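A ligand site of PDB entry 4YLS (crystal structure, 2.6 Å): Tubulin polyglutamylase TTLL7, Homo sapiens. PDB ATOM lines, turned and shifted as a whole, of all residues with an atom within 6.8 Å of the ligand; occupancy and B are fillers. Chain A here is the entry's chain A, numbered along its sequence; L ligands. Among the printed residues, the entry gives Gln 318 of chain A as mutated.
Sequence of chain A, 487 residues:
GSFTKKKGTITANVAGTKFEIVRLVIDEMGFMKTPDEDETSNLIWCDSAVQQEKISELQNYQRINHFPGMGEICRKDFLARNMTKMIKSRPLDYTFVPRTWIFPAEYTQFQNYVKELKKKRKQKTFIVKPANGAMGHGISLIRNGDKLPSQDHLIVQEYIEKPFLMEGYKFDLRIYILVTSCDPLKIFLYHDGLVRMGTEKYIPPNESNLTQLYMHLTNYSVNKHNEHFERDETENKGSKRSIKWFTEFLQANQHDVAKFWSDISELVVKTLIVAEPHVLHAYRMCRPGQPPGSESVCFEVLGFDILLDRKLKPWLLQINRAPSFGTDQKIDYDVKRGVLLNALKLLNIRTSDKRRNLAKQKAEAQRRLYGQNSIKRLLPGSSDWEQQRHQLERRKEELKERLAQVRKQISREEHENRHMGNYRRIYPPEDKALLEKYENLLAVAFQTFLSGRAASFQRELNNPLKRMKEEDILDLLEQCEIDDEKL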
ATOM      1  N   LYS A  76      17.496 -13.957 -10.821  1.00  0.00           N
ATOM      2  CA  LYS A  76      18.144 -15.142 -10.267  1.00  0.00           C
ATOM      3  C   LYS A  76      17.294 -15.829  -9.205  1.00  0.00           C
ATOM      4  O   LYS A  76      17.242 -17.053  -9.137  1.00  0.00           O
ATOM      5  CB  LYS A  76      19.511 -14.774  -9.685  1.00  0.00           C
ATOM      6  CG  LYS A  76      20.457 -14.123 -10.688  1.00  0.00           C
ATOM      7  N   PRO A  98      21.771 -26.141 -11.431  1.00  0.00           N
ATOM      8  CA  PRO A  98      22.486 -26.384 -10.179  1.00  0.00           C
ATOM      9  C   PRO A  98      21.590 -26.166  -8.971  1.00  0.00           C
ATOM     10  O   PRO A  98      20.731 -25.283  -9.016  1.00  0.00           O
ATOM     11  CB  PRO A  98      23.628 -25.366 -10.208  1.00  0.00           C
ATOM     12  CG  PRO A  98      23.762 -24.968 -11.648  1.00  0.00           C
ATOM     13  CD  PRO A  98      22.379 -25.045 -12.214  1.00  0.00           C
ATOM     14  N   ARG A  99      21.769 -26.954  -7.921  1.00  0.00           N
ATOM     15  CA  ARG A  99      20.973 -26.821  -6.705  1.00  0.00           C
ATOM     16  C   ARG A  99      21.116 -25.415  -6.137  1.00  0.00           C
ATOM     17  O   ARG A  99      22.230 -24.958  -5.848  1.00  0.00           O
ATOM     18  CB  ARG A  99      21.386 -27.860  -5.667  1.00  0.00           C
ATOM     19  N   ILE A 127      28.664 -21.756  -4.100  1.00  0.00           N
ATOM     20  CA  ILE A 127      28.932 -20.387  -4.517  1.00  0.00           C
ATOM     21  C   ILE A 127      27.809 -19.457  -4.078  1.00  0.00           C
ATOM     22  O   ILE A 127      26.637 -19.829  -4.083  1.00  0.00           O
ATOM     23  CB  ILE A 127      29.136 -20.300  -6.048  1.00  0.00           C
ATOM     24  CG1 ILE A 127      29.600 -18.892  -6.463  1.00  0.00           C
ATOM     25  CG2 ILE A 127      27.868 -20.701  -6.798  1.00  0.00           C
ATOM     26  CD1 ILE A 127      29.875 -18.747  -7.938  1.00  0.00           C
ATOM     27  N   VAL A 128      28.178 -18.244  -3.667  1.00  0.00           N
ATOM     28  CA  VAL A 128      27.205 -17.240  -3.255  1.00  0.00           C
ATOM     29  C   VAL A 128      27.187 -16.065  -4.232  1.00  0.00           C
ATOM     30  O   VAL A 128      28.246 -15.554  -4.606  1.00  0.00           O
ATOM     31  CB  VAL A 128      27.485 -16.719  -1.832  1.00  0.00           C
ATOM     32  CG1 VAL A 128      26.757 -17.574  -0.802  1.00  0.00           C
ATOM     33  CG2 VAL A 128      28.994 -16.709  -1.564  1.00  0.00           C
ATOM     34  N   LYS A 129      25.995 -15.646  -4.635  1.00  0.00           N
ATOM     35  CA  LYS A 129      25.864 -14.556  -5.595  1.00  0.00           C
ATOM     36  C   LYS A 129      25.039 -13.406  -5.030  1.00  0.00           C
ATOM     37  O   LYS A 129      24.709 -13.407  -3.846  1.00  0.00           O
ATOM     38  CB  LYS A 129      25.222 -15.073  -6.892  1.00  0.00           C
ATOM     39  CG  LYS A 129      25.877 -16.333  -7.445  1.00  0.00           C
ATOM     40  CD  LYS A 129      25.128 -16.874  -8.645  1.00  0.00           C
ATOM     41  CE  LYS A 129      25.778 -18.136  -9.175  1.00  0.00           C
ATOM     42  NZ  LYS A 129      25.040 -18.688 -10.342  1.00  0.00           N
ATOM     43  N   PRO A 130      24.707 -12.419  -5.882  1.00  0.00           N
ATOM     44  CA  PRO A 130      23.933 -11.242  -5.458  1.00  0.00           C
ATOM     45  C   PRO A 130      22.486 -11.598  -5.128  1.00  0.00           C
ATOM     46  O   PRO A 130      21.645 -11.589  -6.021  1.00  0.00           O
ATOM     47  CB  PRO A 130      24.009 -10.321  -6.678  1.00  0.00           C
ATOM     48  N   ILE A 139      30.615 -11.974  -5.061  1.00  0.00           N
ATOM     49  CA  ILE A 139      30.552 -13.404  -5.365  1.00  0.00           C
ATOM     50  C   ILE A 139      31.708 -14.137  -4.696  1.00  0.00           C
ATOM     51  O   ILE A 139      32.875 -13.785  -4.906  1.00  0.00           O
ATOM     52  CB  ILE A 139      30.562 -13.676  -6.884  1.00  0.00           C
ATOM     53  CG1 ILE A 139      29.208 -13.333  -7.523  1.00  0.00           C
ATOM     54  CG2 ILE A 139      30.880 -15.135  -7.154  1.00  0.00           C
ATOM     55  CD1 ILE A 139      28.952 -11.845  -7.705  1.00  0.00           C
ATOM     56  N   GLN A 157      24.353 -21.601  -4.121  1.00  0.00           N
ATOM     57  CA  GLN A 157      24.184 -22.533  -5.232  1.00  0.00           C
ATOM     58  C   GLN A 157      25.326 -23.544  -5.283  1.00  0.00           C
ATOM     59  O   GLN A 157      26.468 -23.226  -4.962  1.00  0.00           O
ATOM     60  CB  GLN A 157      24.112 -21.764  -6.554  1.00  0.00           C
ATOM     61  CG  GLN A 157      23.784 -22.634  -7.751  1.00  0.00           C
ATOM     62  CD  GLN A 157      23.767 -21.848  -9.040  1.00  0.00           C
ATOM     63  OE1 GLN A 157      24.801 -21.337  -9.488  1.00  0.00           O
ATOM     64  NE2 GLN A 157      22.596 -21.732  -9.652  1.00  0.00           N
ATOM     65  N   GLU A 158      25.002 -24.773  -5.678  1.00  0.00           N
ATOM     66  CA  GLU A 158      26.000 -25.815  -5.859  1.00  0.00           C
ATOM     67  C   GLU A 158      26.994 -25.431  -6.948  1.00  0.00           C
ATOM     68  O   GLU A 158      26.607 -24.962  -8.014  1.00  0.00           O
ATOM     69  CB  GLU A 158      25.331 -27.149  -6.198  1.00  0.00           C
ATOM     70  N   TYR A 159      28.272 -25.632  -6.660  1.00  0.00           N
ATOM     71  CA  TYR A 159      29.334 -25.231  -7.572  1.00  0.00           C
ATOM     72  C   TYR A 159      29.768 -26.393  -8.469  1.00  0.00           C
ATOM     73  O   TYR A 159      30.204 -27.425  -7.980  1.00  0.00           O
ATOM     74  CB  TYR A 159      30.544 -24.693  -6.774  1.00  0.00           C
ATOM     75  CG  TYR A 159      31.677 -24.163  -7.627  1.00  0.00           C
ATOM     76  CD1 TYR A 159      31.613 -22.910  -8.206  1.00  0.00           C
ATOM     77  CD2 TYR A 159      32.834 -24.915  -7.828  1.00  0.00           C
ATOM     78  CE1 TYR A 159      32.651 -22.410  -8.980  1.00  0.00           C
ATOM     79  CE2 TYR A 159      33.882 -24.430  -8.592  1.00  0.00           C
ATOM     80  CZ  TYR A 159      33.785 -23.177  -9.164  1.00  0.00           C
ATOM     81  OH  TYR A 159      34.819 -22.689  -9.932  1.00  0.00           O
ATOM     82  N   ILE A 160      29.620 -26.200  -9.780  1.00  0.00           N
ATOM     83  CA  ILE A 160      30.081 -27.208 -10.735  1.00  0.00           C
ATOM     84  C   ILE A 160      31.603 -27.252 -10.669  1.00  0.00           C
ATOM     85  O   ILE A 160      32.281 -26.313 -11.116  1.00  0.00           O
ATOM     86  CB  ILE A 160      29.586 -26.908 -12.173  1.00  0.00           C
ATOM     87  CG1 ILE A 160      28.094 -27.191 -12.336  1.00  0.00           C
ATOM     88  CG2 ILE A 160      30.322 -27.781 -13.177  1.00  0.00           C
ATOM     89  CD1 ILE A 160      27.176 -26.204 -11.668  1.00  0.00           C
ATOM     90  N   GLU A 161      32.138 -28.317 -10.099  1.00  0.00           N
ATOM     91  CA  GLU A 161      33.557 -28.368  -9.745  1.00  0.00           C
ATOM     92  C   GLU A 161      34.461 -28.788 -10.895  1.00  0.00           C
ATOM     93  O   GLU A 161      35.619 -28.366 -10.961  1.00  0.00           O
ATOM     94  CB  GLU A 161      33.766 -29.304  -8.561  1.00  0.00           C
ATOM     95  CG  GLU A 161      33.028 -28.885  -7.304  1.00  0.00           C
ATOM     96  CD  GLU A 161      33.287 -29.818  -6.140  1.00  0.00           C
ATOM     97  OE1 GLU A 161      32.919 -29.459  -4.998  1.00  0.00           O
ATOM     98  OE2 GLU A 161      33.847 -30.901  -6.366  1.00  0.00           O
ATOM     99  N   PRO A 163      34.412 -28.392 -14.636  1.00  0.00           N
ATOM    100  CA  PRO A 163      33.901 -27.856 -15.904  1.00  0.00           C
ATOM    101  C   PRO A 163      34.763 -28.276 -17.096  1.00  0.00           C
ATOM    102  O   PRO A 163      35.910 -28.660 -16.912  1.00  0.00           O
ATOM    103  CB  PRO A 163      33.966 -26.349 -15.686  1.00  0.00           C
ATOM    104  CG  PRO A 163      35.150 -26.163 -14.798  1.00  0.00           C
ATOM    105  CD  PRO A 163      35.177 -27.381 -13.889  1.00  0.00           C
ATOM    106  N   LYS A 170      39.019 -22.613 -17.681  1.00  0.00           N
ATOM    107  CA  LYS A 170      37.569 -22.610 -17.520  1.00  0.00           C
ATOM    108  C   LYS A 170      36.965 -21.469 -18.327  1.00  0.00           C
ATOM    109  O   LYS A 170      37.448 -20.339 -18.265  1.00  0.00           O
ATOM    110  CB  LYS A 170      37.189 -22.475 -16.047  1.00  0.00           C
ATOM    111  CG  LYS A 170      35.704 -22.298 -15.787  1.00  0.00           C
ATOM    112  CD  LYS A 170      35.427 -22.160 -14.301  1.00  0.00           C
ATOM    113  CE  LYS A 170      33.949 -21.986 -14.014  1.00  0.00           C
ATOM    114  NZ  LYS A 170      33.685 -21.884 -12.552  1.00  0.00           N
ATOM    115  N   PHE A 171      35.921 -21.757 -19.095  1.00  0.00           N
ATOM    116  CA  PHE A 171      35.308 -20.746 -19.940  1.00  0.00           C
ATOM    117  C   PHE A 171      33.793 -20.664 -19.730  1.00  0.00           C
ATOM    118  O   PHE A 171      33.189 -21.575 -19.172  1.00  0.00           O
ATOM    119  CB  PHE A 171      35.611 -21.026 -21.414  1.00  0.00           C
ATOM    120  CG  PHE A 171      35.095 -22.338 -21.913  1.00  0.00           C
ATOM    121  CD1 PHE A 171      33.836 -22.439 -22.483  1.00  0.00           C
ATOM    122  CD2 PHE A 171      35.868 -23.487 -21.818  1.00  0.00           C
ATOM    123  CE1 PHE A 171      33.358 -23.651 -22.933  1.00  0.00           C
ATOM    124  CE2 PHE A 171      35.400 -24.700 -22.278  1.00  0.00           C
ATOM    125  CZ  PHE A 171      34.139 -24.790 -22.832  1.00  0.00           C
ATOM    126  N   ASP A 172      33.205 -19.564 -20.186  1.00  0.00           N
ATOM    127  CA  ASP A 172      31.768 -19.353 -20.072  1.00  0.00           C
ATOM    128  C   ASP A 172      31.115 -19.258 -21.449  1.00  0.00           C
ATOM    129  O   ASP A 172      31.725 -18.778 -22.400  1.00  0.00           O
ATOM    130  CB  ASP A 172      31.475 -18.079 -19.276  1.00  0.00           C
ATOM    131  CG  ASP A 172      30.992 -18.377 -17.875  1.00  0.00           C
ATOM    132  OD1 ASP A 172      31.845 -18.525 -16.975  1.00  0.00           O
ATOM    133  OD2 ASP A 172      29.762 -18.444 -17.675  1.00  0.00           O
ATOM    134  N   ARG A 174      28.084 -17.637 -23.602  1.00  0.00           N
ATOM    135  CA  ARG A 174      26.998 -16.681 -23.771  1.00  0.00           C
ATOM    136  C   ARG A 174      26.310 -16.957 -25.096  1.00  0.00           C
ATOM    137  O   ARG A 174      26.819 -16.611 -26.165  1.00  0.00           O
ATOM    138  CB  ARG A 174      27.510 -15.245 -23.710  1.00  0.00           C
ATOM    139  CG  ARG A 174      26.560 -14.178 -24.265  1.00  0.00           C
ATOM    140  CD  ARG A 174      25.258 -14.091 -23.482  1.00  0.00           C
ATOM    141  NE  ARG A 174      25.475 -13.666 -22.101  1.00  0.00           N
ATOM    142  CZ  ARG A 174      25.554 -12.395 -21.706  1.00  0.00           C
ATOM    143  NH1 ARG A 174      25.437 -11.422 -22.591  1.00  0.00           N
ATOM    144  NH2 ARG A 174      25.754 -12.111 -20.428  1.00  0.00           N
ATOM    145  N   ARG A 196      33.988 -16.838 -23.031  1.00  0.00           N
ATOM    146  CA  ARG A 196      34.835 -16.076 -22.126  1.00  0.00           C
ATOM    147  C   ARG A 196      35.765 -16.985 -21.316  1.00  0.00           C
ATOM    148  O   ARG A 196      35.392 -17.469 -20.248  1.00  0.00           O
ATOM    149  CB  ARG A 196      33.981 -15.234 -21.178  1.00  0.00           C
ATOM    150  N   ASP A 305      23.544 -17.443 -20.053  1.00  0.00           N
ATOM    151  CA  ASP A 305      24.875 -17.792 -19.557  1.00  0.00           C
ATOM    152  C   ASP A 305      24.920 -19.264 -19.188  1.00  0.00           C
ATOM    153  O   ASP A 305      24.148 -19.732 -18.350  1.00  0.00           O
ATOM    154  CB  ASP A 305      25.256 -16.915 -18.358  1.00  0.00           C
ATOM    155  CG  ASP A 305      25.453 -15.458 -18.746  1.00  0.00           C
ATOM    156  OD1 ASP A 305      25.743 -15.190 -19.927  1.00  0.00           O
ATOM    157  OD2 ASP A 305      25.310 -14.593 -17.860  1.00  0.00           O
ATOM    158  N   LEU A 307      27.405 -22.912 -18.465  1.00  0.00           N
ATOM    159  CA  LEU A 307      28.679 -23.571 -18.197  1.00  0.00           C
ATOM    160  C   LEU A 307      28.602 -25.058 -18.550  1.00  0.00           C
ATOM    161  O   LEU A 307      27.647 -25.746 -18.205  1.00  0.00           O
ATOM    162  CB  LEU A 307      29.067 -23.394 -16.732  1.00  0.00           C
ATOM    163  CG  LEU A 307      30.327 -24.143 -16.289  1.00  0.00           C
ATOM    164  CD1 LEU A 307      31.559 -23.636 -17.030  1.00  0.00           C
ATOM    165  CD2 LEU A 307      30.531 -24.034 -14.780  1.00  0.00           C
ATOM    166  N   LEU A 316      22.701 -24.305 -16.792  1.00  0.00           N
ATOM    167  CA  LEU A 316      22.171 -22.948 -16.844  1.00  0.00           C
ATOM    168  C   LEU A 316      22.590 -22.158 -15.608  1.00  0.00           C
ATOM    169  O   LEU A 316      22.295 -22.550 -14.480  1.00  0.00           O
ATOM    170  CB  LEU A 316      20.649 -22.970 -16.963  1.00  0.00           C
ATOM    171  CG  LEU A 316      19.961 -21.601 -16.864  1.00  0.00           C
ATOM    172  CD1 LEU A 316      20.268 -20.738 -18.075  1.00  0.00           C
ATOM    173  CD2 LEU A 316      18.461 -21.768 -16.685  1.00  0.00           C
ATOM    174  N   LEU A 317      23.262 -21.032 -15.828  1.00  0.00           N
ATOM    175  CA  LEU A 317      23.693 -20.179 -14.727  1.00  0.00           C
ATOM    176  C   LEU A 317      22.698 -19.054 -14.490  1.00  0.00           C
ATOM    177  O   LEU A 317      22.175 -18.899 -13.383  1.00  0.00           O
ATOM    178  CB  LEU A 317      25.094 -19.614 -14.994  1.00  0.00           C
ATOM    179  CG  LEU A 317      26.200 -20.660 -15.158  1.00  0.00           C
ATOM    180  CD1 LEU A 317      27.572 -19.989 -15.234  1.00  0.00           C
ATOM    181  CD2 LEU A 317      26.156 -21.674 -14.018  1.00  0.00           C
ATOM    182  N   GLN A 318      22.427 -18.261 -15.532  1.00  0.00           N
ATOM    183  CA  GLN A 318      21.425 -17.208 -15.466  1.00  0.00           C
ATOM    184  C   GLN A 318      21.014 -16.739 -16.857  1.00  0.00           C
ATOM    185  O   GLN A 318      21.703 -17.003 -17.837  1.00  0.00           O
ATOM    186  CB  GLN A 318      21.947 -16.021 -14.648  1.00  0.00           C
ATOM    187  CG  GLN A 318      22.983 -15.172 -15.358  1.00  0.00           C
ATOM    188  CD  GLN A 318      23.508 -14.044 -14.491  1.00  0.00           C
ATOM    189  OE1 GLN A 318      23.287 -14.027 -13.279  1.00  0.00           O
ATOM    190  NE2 GLN A 318      24.210 -13.100 -15.105  1.00  0.00           N
HETATM  191  P1  LIG L   1      28.251 -11.932 -13.779  1.00  0.00           P
HETATM  192  O1  LIG L   1      27.183 -11.517 -14.698  1.00  0.00           O
HETATM  193  O2  LIG L   1      28.409 -10.886 -12.729  1.00  0.00           O
HETATM  194  N1  LIG L   1      29.512 -12.062 -14.528  1.00  0.00           N
HETATM  195  P2  LIG L   1      28.174 -13.815 -11.673  1.00  0.00           P
HETATM  196  O3  LIG L   1      28.602 -12.631 -10.758  1.00  0.00           O
HETATM  197  O4  LIG L   1      26.913 -14.465 -11.107  1.00  0.00           O
HETATM  198  O5  LIG L   1      27.879 -13.317 -13.162  1.00  0.00           O
HETATM  199  O6  LIG L   1      29.395 -14.936 -11.714  1.00  0.00           O
HETATM  200  C1  LIG L   1      29.815 -15.447 -12.979  1.00  0.00           C
HETATM  201  C2  LIG L   1      30.902 -16.332 -12.807  1.00  0.00           C
HETATM  202  O7  LIG L   1      30.601 -17.346 -11.713  1.00  0.00           O
HETATM  203  C3  LIG L   1      31.129 -17.166 -14.142  1.00  0.00           C
HETATM  204  O8  LIG L   1      32.529 -16.984 -14.654  1.00  0.00           O
HETATM  205  C4  LIG L   1      30.924 -18.383 -13.837  1.00  0.00           C
HETATM  206  O9  LIG L   1      31.951 -19.216 -14.422  1.00  0.00           O
HETATM  207  C5  LIG L   1      31.014 -18.501 -12.199  1.00  0.00           C
HETATM  208  N2  LIG L   1      30.271 -19.623 -11.740  1.00  0.00           N
HETATM  209  C6  LIG L   1      29.179 -18.890 -11.352  1.00  0.00           C
HETATM  210  N3  LIG L   1      28.259 -19.776 -10.852  1.00  0.00           N
HETATM  211  C7  LIG L   1      28.782 -21.036 -10.946  1.00  0.00           C
HETATM  212  C8  LIG L   1      28.273 -22.301 -10.580  1.00  0.00           C
HETATM  213  N4  LIG L   1      27.035 -22.715  -9.993  1.00  0.00           N
HETATM  214  N5  LIG L   1      29.018 -23.410 -10.788  1.00  0.00           N
HETATM  215  C9  LIG L   1      30.283 -23.298 -11.358  1.00  0.00           C
HETATM  216  N6  LIG L   1      30.776 -22.085 -11.705  1.00  0.00           N
HETATM  217  C10 LIG L   1      30.024 -20.939 -11.497  1.00  0.00           C
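Merely in contact with the ligand: Ile 139 (3.2 Å), Tyr 159 (3.3 Å), Ile 127 (3.5 Å), Leu 307 (3.5 Å) and Leu 317 (3.97 Å).
The side-chain carboxylate (OD1) of Asp 172 is in hydrogen-bond range of an oxygen (O9) of the ligand (2.6 Å).
OE1 of Gln 157 lies within hydrogen-bond range of N4 of the ligand (2.7 Å).
The backbone carbonyl oxygen (O) of Glu 158 sits at hydrogen-bond distance from a nitrogen (N4) of the ligand, at 3.0 Å.
N5 of the ligand is in hydrogen-bond range of N of Ile 160 (3.0 Å).
A nitrogen (N6) of the ligand lies within hydrogen-bond range of the side-chain amino group (NZ) of Lys 170.
An oxygen (O1) of the ligand is in hydrogen-bond range of the side-chain amide nitrogen (NE2) of Gln 318, 3.4 Å away.
The side-chain amino group (NZ) of Lys 129 lies close to a nitrogen (N3) of the ligand (3.4 Å).
N of Asp 172 sits at hydrogen-bond distance from O of Arg 196, at 3.0 Å.
NZ of Lys 129 is in hydrogen-bond range of OE1 of Gln 157 (2.8 Å).
The backbone carbonyl oxygen (O) of Gln 157 is in hydrogen-bond range of the backbone NH (N) of Ile 127, 2.8 Å away.
O of Arg 99 sits at hydrogen-bond distance from N of Glu 158 (2.8 Å).
The side-chain hydroxyl (OH) of Tyr 159 is in hydrogen-bond range of the side-chain amino group (NZ) of Lys 170, 3.0 Å away.
The backbone carbonyl oxygen of Gln 318 sits at hydrogen-bond distance from the backbone NH of Asp 305 (2.9 Å).
O of Asp 305 sits at hydrogen-bond distance from N of Leu 317 (3.0 Å).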
